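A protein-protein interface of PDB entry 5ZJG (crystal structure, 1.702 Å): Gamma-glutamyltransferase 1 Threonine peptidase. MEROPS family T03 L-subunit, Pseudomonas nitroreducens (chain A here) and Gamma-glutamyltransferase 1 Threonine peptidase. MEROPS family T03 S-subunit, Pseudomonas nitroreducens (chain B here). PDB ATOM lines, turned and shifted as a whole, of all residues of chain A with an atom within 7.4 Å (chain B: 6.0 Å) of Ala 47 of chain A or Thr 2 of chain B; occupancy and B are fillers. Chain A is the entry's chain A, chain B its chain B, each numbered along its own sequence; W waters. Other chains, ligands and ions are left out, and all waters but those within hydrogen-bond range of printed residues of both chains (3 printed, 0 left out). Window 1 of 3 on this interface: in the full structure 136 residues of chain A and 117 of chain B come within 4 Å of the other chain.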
ATOM      1  N   ALA A  10      20.410  19.689   5.277  1.00  0.00           N
ATOM      2  CA  ALA A  10      21.462  19.696   6.282  1.00  0.00           C
ATOM      3  C   ALA A  10      21.722  21.124   6.753  1.00  0.00           C
ATOM      4  O   ALA A  10      21.421  22.076   6.039  1.00  0.00           O
ATOM      5  CB  ALA A  10      22.756  19.108   5.711  1.00  0.00           C
ATOM      6  N   PRO A  11      22.280  21.298   7.948  1.00  0.00           N
ATOM      7  CA  PRO A  11      22.444  22.650   8.506  1.00  0.00           C
ATOM      8  C   PRO A  11      23.621  23.427   7.943  1.00  0.00           C
ATOM      9  O   PRO A  11      23.755  24.613   8.260  1.00  0.00           O
ATOM     10  CB  PRO A  11      22.627  22.378  10.000  1.00  0.00           C
ATOM     11  CG  PRO A  11      23.311  21.057  10.019  1.00  0.00           C
ATOM     12  CD  PRO A  11      22.628  20.266   8.929  1.00  0.00           C
ATOM     13  N   ASP A  12      24.448  22.837   7.081  1.00  0.00           N
ATOM     14  CA  ASP A  12      25.405  23.639   6.329  1.00  0.00           C
ATOM     15  C   ASP A  12      25.652  22.963   4.977  1.00  0.00           C
ATOM     16  O   ASP A  12      25.100  21.894   4.672  1.00  0.00           O
ATOM     17  CB  ASP A  12      26.673  23.923   7.173  1.00  0.00           C
ATOM     18  CG  ASP A  12      27.658  22.760   7.250  1.00  0.00           C
ATOM     19  OD1 ASP A  12      27.513  21.741   6.531  1.00  0.00           O
ATOM     20  OD2 ASP A  12      28.586  22.850   8.102  1.00  0.00           O
ATOM     21  N   LEU A  40      29.745  17.118  10.010  1.00  0.00           N
ATOM     22  CA  LEU A  40      29.357  18.275  10.797  1.00  0.00           C
ATOM     23  C   LEU A  40      30.124  18.343  12.109  1.00  0.00           C
ATOM     24  O   LEU A  40      30.268  19.430  12.676  1.00  0.00           O
ATOM     25  CB  LEU A  40      27.851  18.248  11.050  1.00  0.00           C
ATOM     26  CG  LEU A  40      26.944  18.368   9.818  1.00  0.00           C
ATOM     27  CD1 LEU A  40      25.483  18.055  10.219  1.00  0.00           C
ATOM     28  CD2 LEU A  40      27.056  19.747   9.186  1.00  0.00           C
ATOM     29  N   ALA A  41      30.675  17.218  12.566  1.00  0.00           N
ATOM     30  CA  ALA A  41      31.581  17.264  13.708  1.00  0.00           C
ATOM     31  C   ALA A  41      32.858  18.021  13.399  1.00  0.00           C
ATOM     32  O   ALA A  41      33.577  18.425  14.330  1.00  0.00           O
ATOM     33  CB  ALA A  41      31.926  15.847  14.157  1.00  0.00           C
ATOM     34  N   TYR A  44      30.833  22.045  11.743  1.00  0.00           N
ATOM     35  CA  TYR A  44      29.804  22.701  12.549  1.00  0.00           C
ATOM     36  C   TYR A  44      30.129  22.503  14.032  1.00  0.00           C
ATOM     37  O   TYR A  44      29.297  22.013  14.799  1.00  0.00           O
ATOM     38  CB  TYR A  44      28.440  22.121  12.176  1.00  0.00           C
ATOM     39  CG  TYR A  44      27.265  23.084  12.241  1.00  0.00           C
ATOM     40  CD1 TYR A  44      26.685  23.430  13.440  1.00  0.00           C
ATOM     41  CD2 TYR A  44      26.708  23.597  11.088  1.00  0.00           C
ATOM     42  CE1 TYR A  44      25.590  24.299  13.484  1.00  0.00           C
ATOM     43  CE2 TYR A  44      25.620  24.468  11.121  1.00  0.00           C
ATOM     44  CZ  TYR A  44      25.076  24.805  12.328  1.00  0.00           C
ATOM     45  OH  TYR A  44      24.004  25.657  12.386  1.00  0.00           O
ATOM     46  N   PRO A  45      31.353  22.856  14.463  1.00  0.00           N
ATOM     47  CA  PRO A  45      31.821  22.447  15.805  1.00  0.00           C
ATOM     48  C   PRO A  45      31.015  23.030  16.951  1.00  0.00           C
ATOM     49  O   PRO A  45      31.132  22.535  18.085  1.00  0.00           O
ATOM     50  CB  PRO A  45      33.277  22.940  15.829  1.00  0.00           C
ATOM     51  CG  PRO A  45      33.318  24.043  14.805  1.00  0.00           C
ATOM     52  CD  PRO A  45      32.439  23.509  13.715  1.00  0.00           C
ATOM     53  N   GLU A  46      30.195  24.050  16.701  1.00  0.00           N
ATOM     54  CA  GLU A  46      29.362  24.582  17.775  1.00  0.00           C
ATOM     55  C   GLU A  46      28.289  23.585  18.197  1.00  0.00           C
ATOM     56  O   GLU A  46      27.750  23.696  19.306  1.00  0.00           O
ATOM     57  CB  GLU A  46      28.731  25.919  17.334  1.00  0.00           C
ATOM     58  CG  GLU A  46      27.827  25.850  16.088  1.00  0.00           C
ATOM     59  CD  GLU A  46      28.569  26.062  14.763  1.00  0.00           C
ATOM     60  OE1 GLU A  46      29.680  25.523  14.600  1.00  0.00           O
ATOM     61  OE2 GLU A  46      28.028  26.777  13.885  1.00  0.00           O
ATOM     62  N   ALA A  47      27.977  22.611  17.349  1.00  0.00           N
ATOM     63  CA  ALA A  47      26.916  21.654  17.635  1.00  0.00           C
ATOM     64  C   ALA A  47      27.199  20.269  17.074  1.00  0.00           C
ATOM     65  O   ALA A  47      27.037  19.273  17.778  1.00  0.00           O
ATOM     66  CB  ALA A  47      25.587  22.135  17.080  1.00  0.00           C
ATOM     67  N   GLY A  48      27.524  20.169  15.789  1.00  0.00           N
ATOM     68  CA  GLY A  48      28.010  18.895  15.281  1.00  0.00           C
ATOM     69  C   GLY A  48      29.202  18.432  16.099  1.00  0.00           C
ATOM     70  O   GLY A  48      30.020  19.239  16.543  1.00  0.00           O
ATOM     71  N   ASN A  49      29.307  17.124  16.310  1.00  0.00           N
ATOM     72  CA  ASN A  49      30.211  16.686  17.370  1.00  0.00           C
ATOM     73  C   ASN A  49      30.533  15.206  17.296  1.00  0.00           C
ATOM     74  O   ASN A  49      29.754  14.397  16.782  1.00  0.00           O
ATOM     75  CB  ASN A  49      29.587  16.939  18.743  1.00  0.00           C
ATOM     76  CG  ASN A  49      28.377  16.040  18.968  1.00  0.00           C
ATOM     77  OD1 ASN A  49      28.499  14.936  19.469  1.00  0.00           O
ATOM     78  ND2 ASN A  49      27.210  16.507  18.541  1.00  0.00           N
ATOM     79  N   ILE A  50      31.656  14.864  17.935  1.00  0.00           N
ATOM     80  CA  ILE A  50      31.886  13.526  18.467  1.00  0.00           C
ATOM     81  C   ILE A  50      31.949  13.519  19.996  1.00  0.00           C
ATOM     82  O   ILE A  50      32.013  12.430  20.594  1.00  0.00           O
ATOM     83  CB  ILE A  50      33.159  12.880  17.877  1.00  0.00           C
ATOM     84  CG1 ILE A  50      34.402  13.737  18.152  1.00  0.00           C
ATOM     85  CG2 ILE A  50      32.985  12.660  16.374  1.00  0.00           C
ATOM     86  CD1 ILE A  50      35.732  13.024  17.775  1.00  0.00           C
ATOM     87  N   GLY A  51      31.918  14.685  20.646  1.00  0.00           N
ATOM     88  CA  GLY A  51      32.003  14.782  22.089  1.00  0.00           C
ATOM     89  C   GLY A  51      30.688  15.038  22.792  1.00  0.00           C
ATOM     90  O   GLY A  51      30.695  15.322  23.999  1.00  0.00           O
ATOM     91  N   GLY A  52      29.566  14.918  22.089  1.00  0.00           N
ATOM     92  CA  GLY A  52      28.246  15.111  22.652  1.00  0.00           C
ATOM     93  C   GLY A  52      27.381  13.880  22.467  1.00  0.00           C
ATOM     94  O   GLY A  52      27.863  12.752  22.638  1.00  0.00           O
ATOM     95  N   GLY A  53      26.112  14.080  22.135  1.00  0.00           N
ATOM     96  CA  GLY A  53      25.161  12.989  21.987  1.00  0.00           C
ATOM     97  C   GLY A  53      23.947  13.455  21.215  1.00  0.00           C
ATOM     98  O   GLY A  53      23.866  14.598  20.771  1.00  0.00           O
ATOM     99  N   PHE A  55      19.998  11.863  19.131  1.00  0.00           N
ATOM    100  CA  PHE A  55      18.919  10.926  18.858  1.00  0.00           C
ATOM    101  C   PHE A  55      18.752  10.773  17.350  1.00  0.00           C
ATOM    102  O   PHE A  55      18.818  11.764  16.610  1.00  0.00           O
ATOM    103  CB  PHE A  55      17.568  11.423  19.420  1.00  0.00           C
ATOM    104  CG  PHE A  55      17.524  11.621  20.908  1.00  0.00           C
ATOM    105  CD1 PHE A  55      17.898  10.620  21.774  1.00  0.00           C
ATOM    106  CD2 PHE A  55      17.047  12.803  21.437  1.00  0.00           C
ATOM    107  CE1 PHE A  55      17.813  10.806  23.154  1.00  0.00           C
ATOM    108  CE2 PHE A  55      16.975  13.000  22.814  1.00  0.00           C
ATOM    109  CZ  PHE A  55      17.363  11.996  23.668  1.00  0.00           C
ATOM    110  N   THR A 106      27.922  10.075  20.760  1.00  0.00           N
ATOM    111  CA  THR A 106      27.743  10.199  19.310  1.00  0.00           C
ATOM    112  C   THR A 106      28.502   9.123  18.543  1.00  0.00           C
ATOM    113  O   THR A 106      27.948   8.511  17.628  1.00  0.00           O
ATOM    114  CB  THR A 106      28.160  11.591  18.856  1.00  0.00           C
ATOM    115  OG1 THR A 106      27.224  12.525  19.383  1.00  0.00           O
ATOM    116  CG2 THR A 106      28.171  11.717  17.316  1.00  0.00           C
ATOM    117  N   GLN A 143      28.959  31.378  12.878  1.00  0.00           N
ATOM    118  CA  GLN A 143      30.023  30.705  13.623  1.00  0.00           C
ATOM    119  C   GLN A 143      30.961  31.699  14.275  1.00  0.00           C
ATOM    120  O   GLN A 143      31.307  31.564  15.452  1.00  0.00           O
ATOM    121  CB  GLN A 143      30.831  29.807  12.694  1.00  0.00           C
ATOM    122  CG  GLN A 143      30.219  28.508  12.464  1.00  0.00           C
ATOM    123  CD  GLN A 143      31.163  27.558  11.750  1.00  0.00           C
ATOM    124  OE1 GLN A 143      31.945  27.969  10.899  1.00  0.00           O
ATOM    125  NE2 GLN A 143      31.091  26.279  12.103  1.00  0.00           N
ATOM    126  N   THR B   1      23.003  22.720  19.426  1.00  0.00           N
ATOM    127  CA  THR B   1      22.299  21.590  18.807  1.00  0.00           C
ATOM    128  C   THR B   1      22.234  21.809  17.315  1.00  0.00           C
ATOM    129  O   THR B   1      22.241  22.971  16.874  1.00  0.00           O
ATOM    130  CB  THR B   1      20.889  21.474  19.392  1.00  0.00           C
ATOM    131  OG1 THR B   1      20.984  21.404  20.829  1.00  0.00           O
ATOM    132  CG2 THR B   1      20.127  20.268  18.817  1.00  0.00           C
ATOM    133  N   THR B   2      22.124  20.726  16.535  1.00  0.00           N
ATOM    134  CA  THR B   2      21.778  20.860  15.118  1.00  0.00           C
ATOM    135  C   THR B   2      21.020  19.626  14.633  1.00  0.00           C
ATOM    136  O   THR B   2      20.998  18.585  15.287  1.00  0.00           O
ATOM    137  CB  THR B   2      23.012  21.094  14.248  1.00  0.00           C
ATOM    138  OG1 THR B   2      22.586  21.460  12.928  1.00  0.00           O
ATOM    139  CG2 THR B   2      23.908  19.869  14.176  1.00  0.00           C
ATOM    140  N   HIS B   3      20.366  19.762  13.481  1.00  0.00           N
ATOM    141  CA  HIS B   3      19.511  18.701  12.955  1.00  0.00           C
ATOM    142  C   HIS B   3      19.720  18.528  11.459  1.00  0.00           C
ATOM    143  O   HIS B   3      19.884  19.521  10.747  1.00  0.00           O
ATOM    144  CB  HIS B   3      18.017  18.996  13.188  1.00  0.00           C
ATOM    145  CG  HIS B   3      17.129  17.912  12.670  1.00  0.00           C
ATOM    146  ND1 HIS B   3      16.800  16.805  13.419  1.00  0.00           N
ATOM    147  CD2 HIS B   3      16.542  17.734  11.455  1.00  0.00           C
ATOM    148  CE1 HIS B   3      16.077  15.977  12.690  1.00  0.00           C
ATOM    149  NE2 HIS B   3      15.874  16.531  11.500  1.00  0.00           N
ATOM    150  N   PHE B   4      19.638  17.277  10.974  1.00  0.00           N
ATOM    151  CA  PHE B   4      19.579  17.021   9.533  1.00  0.00           C
ATOM    152  C   PHE B   4      18.613  15.876   9.232  1.00  0.00           C
ATOM    153  O   PHE B   4      18.317  15.020  10.071  1.00  0.00           O
ATOM    154  CB  PHE B   4      20.957  16.752   8.942  1.00  0.00           C
ATOM    155  CG  PHE B   4      21.666  15.564   9.509  1.00  0.00           C
ATOM    156  CD1 PHE B   4      21.453  14.292   8.973  1.00  0.00           C
ATOM    157  CD2 PHE B   4      22.592  15.722  10.536  1.00  0.00           C
ATOM    158  CE1 PHE B   4      22.135  13.180   9.497  1.00  0.00           C
ATOM    159  CE2 PHE B   4      23.283  14.621  11.039  1.00  0.00           C
ATOM    160  CZ  PHE B   4      23.053  13.357  10.510  1.00  0.00           C
ATOM    161  N   ASN B  16      17.917  13.162  12.309  1.00  0.00           N
ATOM    162  CA  ASN B  16      18.970  13.083  13.313  1.00  0.00           C
ATOM    163  C   ASN B  16      19.202  14.455  13.943  1.00  0.00           C
ATOM    164  O   ASN B  16      19.582  15.404  13.246  1.00  0.00           O
ATOM    165  CB  ASN B  16      20.271  12.565  12.714  1.00  0.00           C
ATOM    166  CG  ASN B  16      21.285  12.264  13.792  1.00  0.00           C
ATOM    167  OD1 ASN B  16      21.300  11.173  14.314  1.00  0.00           O
ATOM    168  ND2 ASN B  16      22.101  13.240  14.135  1.00  0.00           N
ATOM    169  N   THR B  17      18.993  14.548  15.263  1.00  0.00           N
ATOM    170  CA  THR B  17      19.321  15.743  16.033  1.00  0.00           C
ATOM    171  C   THR B  17      20.446  15.379  16.984  1.00  0.00           C
ATOM    172  O   THR B  17      20.342  14.383  17.704  1.00  0.00           O
ATOM    173  CB  THR B  17      18.110  16.256  16.823  1.00  0.00           C
ATOM    174  OG1 THR B  17      16.912  16.264  15.999  1.00  0.00           O
ATOM    175  CG2 THR B  17      18.401  17.677  17.353  1.00  0.00           C
ATOM    176  N   TYR B  18      21.530  16.155  16.982  1.00  0.00           N
ATOM    177  CA  TYR B  18      22.568  15.867  17.972  1.00  0.00           C
ATOM    178  C   TYR B  18      23.220  17.180  18.384  1.00  0.00           C
ATOM    179  O   TYR B  18      22.933  18.238  17.818  1.00  0.00           O
ATOM    180  CB  TYR B  18      23.554  14.799  17.473  1.00  0.00           C
ATOM    181  CG  TYR B  18      24.538  15.167  16.363  1.00  0.00           C
ATOM    182  CD1 TYR B  18      24.262  16.170  15.422  1.00  0.00           C
ATOM    183  CD2 TYR B  18      25.713  14.460  16.236  1.00  0.00           C
ATOM    184  CE1 TYR B  18      25.190  16.480  14.424  1.00  0.00           C
ATOM    185  CE2 TYR B  18      26.649  14.764  15.253  1.00  0.00           C
ATOM    186  CZ  TYR B  18      26.368  15.753  14.339  1.00  0.00           C
ATOM    187  OH  TYR B  18      27.282  16.075  13.379  1.00  0.00           O
ATOM    188  N   THR B  19      24.021  17.129  19.444  1.00  0.00           N
ATOM    189  CA  THR B  19      24.334  18.385  20.111  1.00  0.00           C
ATOM    190  C   THR B  19      25.485  18.239  21.089  1.00  0.00           C
ATOM    191  O   THR B  19      25.789  17.150  21.573  1.00  0.00           O
ATOM    192  CB  THR B  19      23.101  18.906  20.852  1.00  0.00           C
ATOM    193  OG1 THR B  19      23.354  20.223  21.341  1.00  0.00           O
ATOM    194  CG2 THR B  19      22.733  17.981  21.998  1.00  0.00           C
ATOM    195  N   LEU B  20      26.083  19.391  21.418  1.00  0.00           N
ATOM    196  CA  LEU B  20      26.923  19.558  22.599  1.00  0.00           C
ATOM    197  C   LEU B  20      26.166  20.212  23.747  1.00  0.00           C
ATOM    198  O   LEU B  20      26.719  20.355  24.849  1.00  0.00           O
ATOM    199  CB  LEU B  20      28.129  20.422  22.255  1.00  0.00           C
ATOM    200  CG  LEU B  20      29.170  19.861  21.291  1.00  0.00           C
ATOM    201  CD1 LEU B  20      30.198  20.964  21.028  1.00  0.00           C
ATOM    202  CD2 LEU B  20      29.846  18.625  21.909  1.00  0.00           C
ATOM    203  N   TRP B  22      24.935  23.708  24.668  1.00  0.00           N
ATOM    204  CA  TRP B  22      25.123  25.080  24.219  1.00  0.00           C
ATOM    205  C   TRP B  22      26.220  25.136  23.154  1.00  0.00           C
ATOM    206  O   TRP B  22      26.873  24.141  22.849  1.00  0.00           O
ATOM    207  CB  TRP B  22      25.395  25.985  25.414  1.00  0.00           C
ATOM    208  CG  TRP B  22      24.131  26.119  26.169  1.00  0.00           C
ATOM    209  CD1 TRP B  22      23.700  25.309  27.174  1.00  0.00           C
ATOM    210  CD2 TRP B  22      23.073  27.061  25.925  1.00  0.00           C
ATOM    211  NE1 TRP B  22      22.459  25.708  27.602  1.00  0.00           N
ATOM    212  CE2 TRP B  22      22.051  26.782  26.851  1.00  0.00           C
ATOM    213  CE3 TRP B  22      22.900  28.123  25.025  1.00  0.00           C
ATOM    214  CZ2 TRP B  22      20.875  27.526  26.911  1.00  0.00           C
ATOM    215  CZ3 TRP B  22      21.735  28.863  25.091  1.00  0.00           C
ATOM    216  CH2 TRP B  22      20.733  28.556  26.020  1.00  0.00           C
ATOM    217  N   ASP B  23      26.365  26.305  22.533  1.00  0.00           N
ATOM    218  CA  ASP B  23      27.334  26.458  21.453  1.00  0.00           C
ATOM    219  C   ASP B  23      28.737  26.161  21.960  1.00  0.00           C
ATOM    220  O   ASP B  23      29.223  26.798  22.906  1.00  0.00           O
ATOM    221  CB  ASP B  23      27.264  27.866  20.868  1.00  0.00           C
ATOM    222  CG  ASP B  23      25.913  28.172  20.239  1.00  0.00           C
ATOM    223  OD1 ASP B  23      25.365  27.310  19.519  1.00  0.00           O
ATOM    224  OD2 ASP B  23      25.397  29.273  20.480  1.00  0.00           O
ATOM    225  N   PHE B  24      29.377  25.176  21.333  1.00  0.00           N
ATOM    226  CA  PHE B  24      30.712  24.705  21.689  1.00  0.00           C
ATOM    227  C   PHE B  24      30.739  24.004  23.030  1.00  0.00           C
ATOM    228  O   PHE B  24      31.822  23.808  23.596  1.00  0.00           O
ATOM    229  CB  PHE B  24      31.742  25.843  21.682  1.00  0.00           C
ATOM    230  CG  PHE B  24      31.827  26.569  20.374  1.00  0.00           C
ATOM    231  CD1 PHE B  24      32.393  25.960  19.261  1.00  0.00           C
ATOM    232  CD2 PHE B  24      31.342  27.856  20.250  1.00  0.00           C
ATOM    233  CE1 PHE B  24      32.452  26.627  18.049  1.00  0.00           C
ATOM    234  CE2 PHE B  24      31.411  28.523  19.050  1.00  0.00           C
ATOM    235  CZ  PHE B  24      31.973  27.907  17.951  1.00  0.00           C
ATOM    236  N   MET B  74      15.071  17.298  22.317  1.00  0.00           N
ATOM    237  CA  MET B  74      15.316  17.004  20.907  1.00  0.00           C
ATOM    238  C   MET B  74      14.290  16.001  20.398  1.00  0.00           C
ATOM    239  O   MET B  74      13.978  15.008  21.054  1.00  0.00           O
ATOM    240  CB  MET B  74      16.716  16.443  20.686  1.00  0.00           C
ATOM    241  CG  MET B  74      17.853  17.411  20.995  1.00  0.00           C
ATOM    242  SD  MET B  74      19.457  16.725  20.612  1.00  0.00           S
ATOM    243  CE  MET B  74      19.677  15.592  21.994  1.00  0.00           C
ATOM    244  N   THR B  91      14.817  20.043  14.500  1.00  0.00           N
ATOM    245  CA  THR B  91      15.399  21.358  14.737  1.00  0.00           C
ATOM    246  C   THR B  91      16.194  21.367  16.033  1.00  0.00           C
ATOM    247  O   THR B  91      15.881  20.620  16.963  1.00  0.00           O
ATOM    248  CB  THR B  91      14.315  22.447  14.802  1.00  0.00           C
ATOM    249  OG1 THR B  91      14.936  23.717  15.044  1.00  0.00           O
ATOM    250  CG2 THR B  91      13.293  22.155  15.927  1.00  0.00           C
ATOM    251  N   PRO B  92      17.187  22.239  16.140  1.00  0.00           N
ATOM    252  CA  PRO B  92      17.750  22.595  17.438  1.00  0.00           C
ATOM    253  C   PRO B  92      16.856  23.609  18.130  1.00  0.00           C
ATOM    254  O   PRO B  92      15.854  24.060  17.582  1.00  0.00           O
ATOM    255  CB  PRO B  92      19.083  23.228  17.057  1.00  0.00           C
ATOM    256  CG  PRO B  92      18.776  23.902  15.752  1.00  0.00           C
ATOM    257  CD  PRO B  92      17.912  22.892  15.048  1.00  0.00           C
ATOM    258  N   ASP B 166      16.151  25.901  13.795  1.00  0.00           N
ATOM    259  CA  ASP B 166      16.807  25.793  12.487  1.00  0.00           C
ATOM    260  C   ASP B 166      16.266  24.524  11.837  1.00  0.00           C
ATOM    261  O   ASP B 166      16.926  23.472  11.816  1.00  0.00           O
ATOM    262  CB  ASP B 166      18.329  25.754  12.650  1.00  0.00           C
ATOM    263  CG  ASP B 166      19.089  25.813  11.324  1.00  0.00           C
ATOM    264  OD1 ASP B 166      18.456  25.968  10.266  1.00  0.00           O
ATOM    265  OD2 ASP B 166      20.342  25.707  11.363  1.00  0.00           O
HETATM  266  O   HOH W   1      25.608  22.330  20.555  1.00  0.00           O
HETATM  267  O   HOH W   2      21.783  24.014  13.228  1.00  0.00           O
HETATM  268  O   HOH W   3      22.519  26.212  10.164  1.00  0.00           O
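O of Glu 46 of chain A is in hydrogen-bond range of N of Phe 24 of chain B. O of Phe 55 of chain A lies close to OD1 of Asn 16 of chain B (3.4 Å). The backbone carbonyl oxygen (O) of Thr 17 of chain B is in hydrogen-bond range of the backbone NH (N) of Phe 55 of chain A. The backbone carbonyl oxygen (O) of Gly 53 of chain A is in hydrogen-bond range of the backbone NH (N) of Thr 19 of chain B (2.9 Å). The side-chain amide nitrogen (ND2) of Asn 49 of chain A lies close to the backbone NH (N) of Thr 19 of chain B (3.4 Å).
The side-chain amide oxygen (OD1) of Asn 49 of chain A sits at hydrogen-bond distance from the side-chain hydroxyl (OG1) of Thr 106 of chain A (2.7 Å). OG1 of Thr 91 of chain B lies within hydrogen-bond range of N of Asp 166 of chain B (2.8 Å). The backbone NH of Gly 53 of chain A is in hydrogen-bond range of the side-chain hydroxyl of Thr 106 of chain A, 3.4 Å away. A ring nitrogen (ND1) of His 3 of chain B is in hydrogen-bond range of the side-chain hydroxyl of Thr 17 of chain B (2.6 Å). The side-chain carboxylate of Glu 46 of chain A sits at hydrogen-bond distance from the side-chain amide nitrogen of Gln 143 of chain A (3.0 Å). The backbone carbonyl oxygen (O) of Asn 16 of chain B is in hydrogen-bond range of a ring nitrogen (ND1) of His 3 of chain B (3.1 Å).
Phe 4 of chain B touches Pro 11 of chain A. CD1 of Leu 40 of chain A touches CD2 of Phe 4 of chain B (3.7 Å). Leu 40 of chain A touches Tyr 18 of chain B (CB to OH, 3.2 Å). Ala 41 of chain A touches Tyr 18 of chain B (N to OH, 3.7 Å). Pro 45 of chain A touches Leu 20 of chain B (O to CD1, 3.5 Å). Ala 47 of chain A touches Thr 1 of chain B (CB to C, 3.4 Å). Gly 52 of chain A touches Leu 20 of chain B. O of Gly 53 of chain A touches CB of Tyr 18 of chain B, at 3.3 Å. CB of Met 74 of chain B touches CD2 of Phe 55 of chain A (3.7 Å). Tyr 18 of chain B touches Thr 106 of chain A (CD2 to CG2, 3.8 Å).
Printed residues of chain B within 4 Å of Ala 10 of chain A: Phe 4 (3.9997 Å). Printed residues of chain B within 4 Å of Ala 41 of chain A: Tyr 18 (3.7 Å). Ala 47 of chain A touches just these residues of chain B: Thr 1 (3.4 Å), Thr 2 (3.8 Å), Thr 19 (3.7 Å) and Leu 20 (3.8 Å). Printed residues of chain B within 4 Å of Asn 49 of chain A: Tyr 18 (3.4 Å), Thr 19 (3.4 Å) and Leu 20 (3.6 Å). Of chain A, only Pro 11 (3.0 Å), Ala 47 (3.8 Å) and Gly 48 (3.97 Å) come within 4 Å of Thr 2 of chain B. The nearest residue of chain B that does not touch Ala 47 of chain A is Tyr 18 of chain B (4.2 Å). The nearest residue of chain A that does not touch Thr 2 of chain B is Tyr 44 of chain A (4.2 Å).
Of the 16 printed residues of chain B, 14 touch a printed residue of chain A. Hydrophobic or aromatic side chains of chain B that line the printed part of chain A: Phe 4, Tyr 18, Leu 20, Phe 24 and Met 74. Along chain B the printed residues that touch a printed residue of chain A span positions 1 to 166.
Water W3 lies within hydrogen-bond range of OD2 of Asp 166 of chain B (2.5 Å), OH of Tyr 44 of chain A (2.7 Å) and O of Pro 11 of chain A (2.8 Å). Water W2 lies within hydrogen-bond range of the side-chain hydroxyl of Thr 2 of chain B (2.7 Å), the side-chain hydroxyl of Tyr 44 of chain A (2.9 Å) and the side-chain carboxylate of Asp 166 of chain B (2.9 Å). Water W1 lies within hydrogen-bond range of O of Glu 46 of chain A, N of Thr 1 of chain B, N of Leu 20 of chain B, OG1 of Thr 19 of chain B and O of Trp 22 of chain B.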
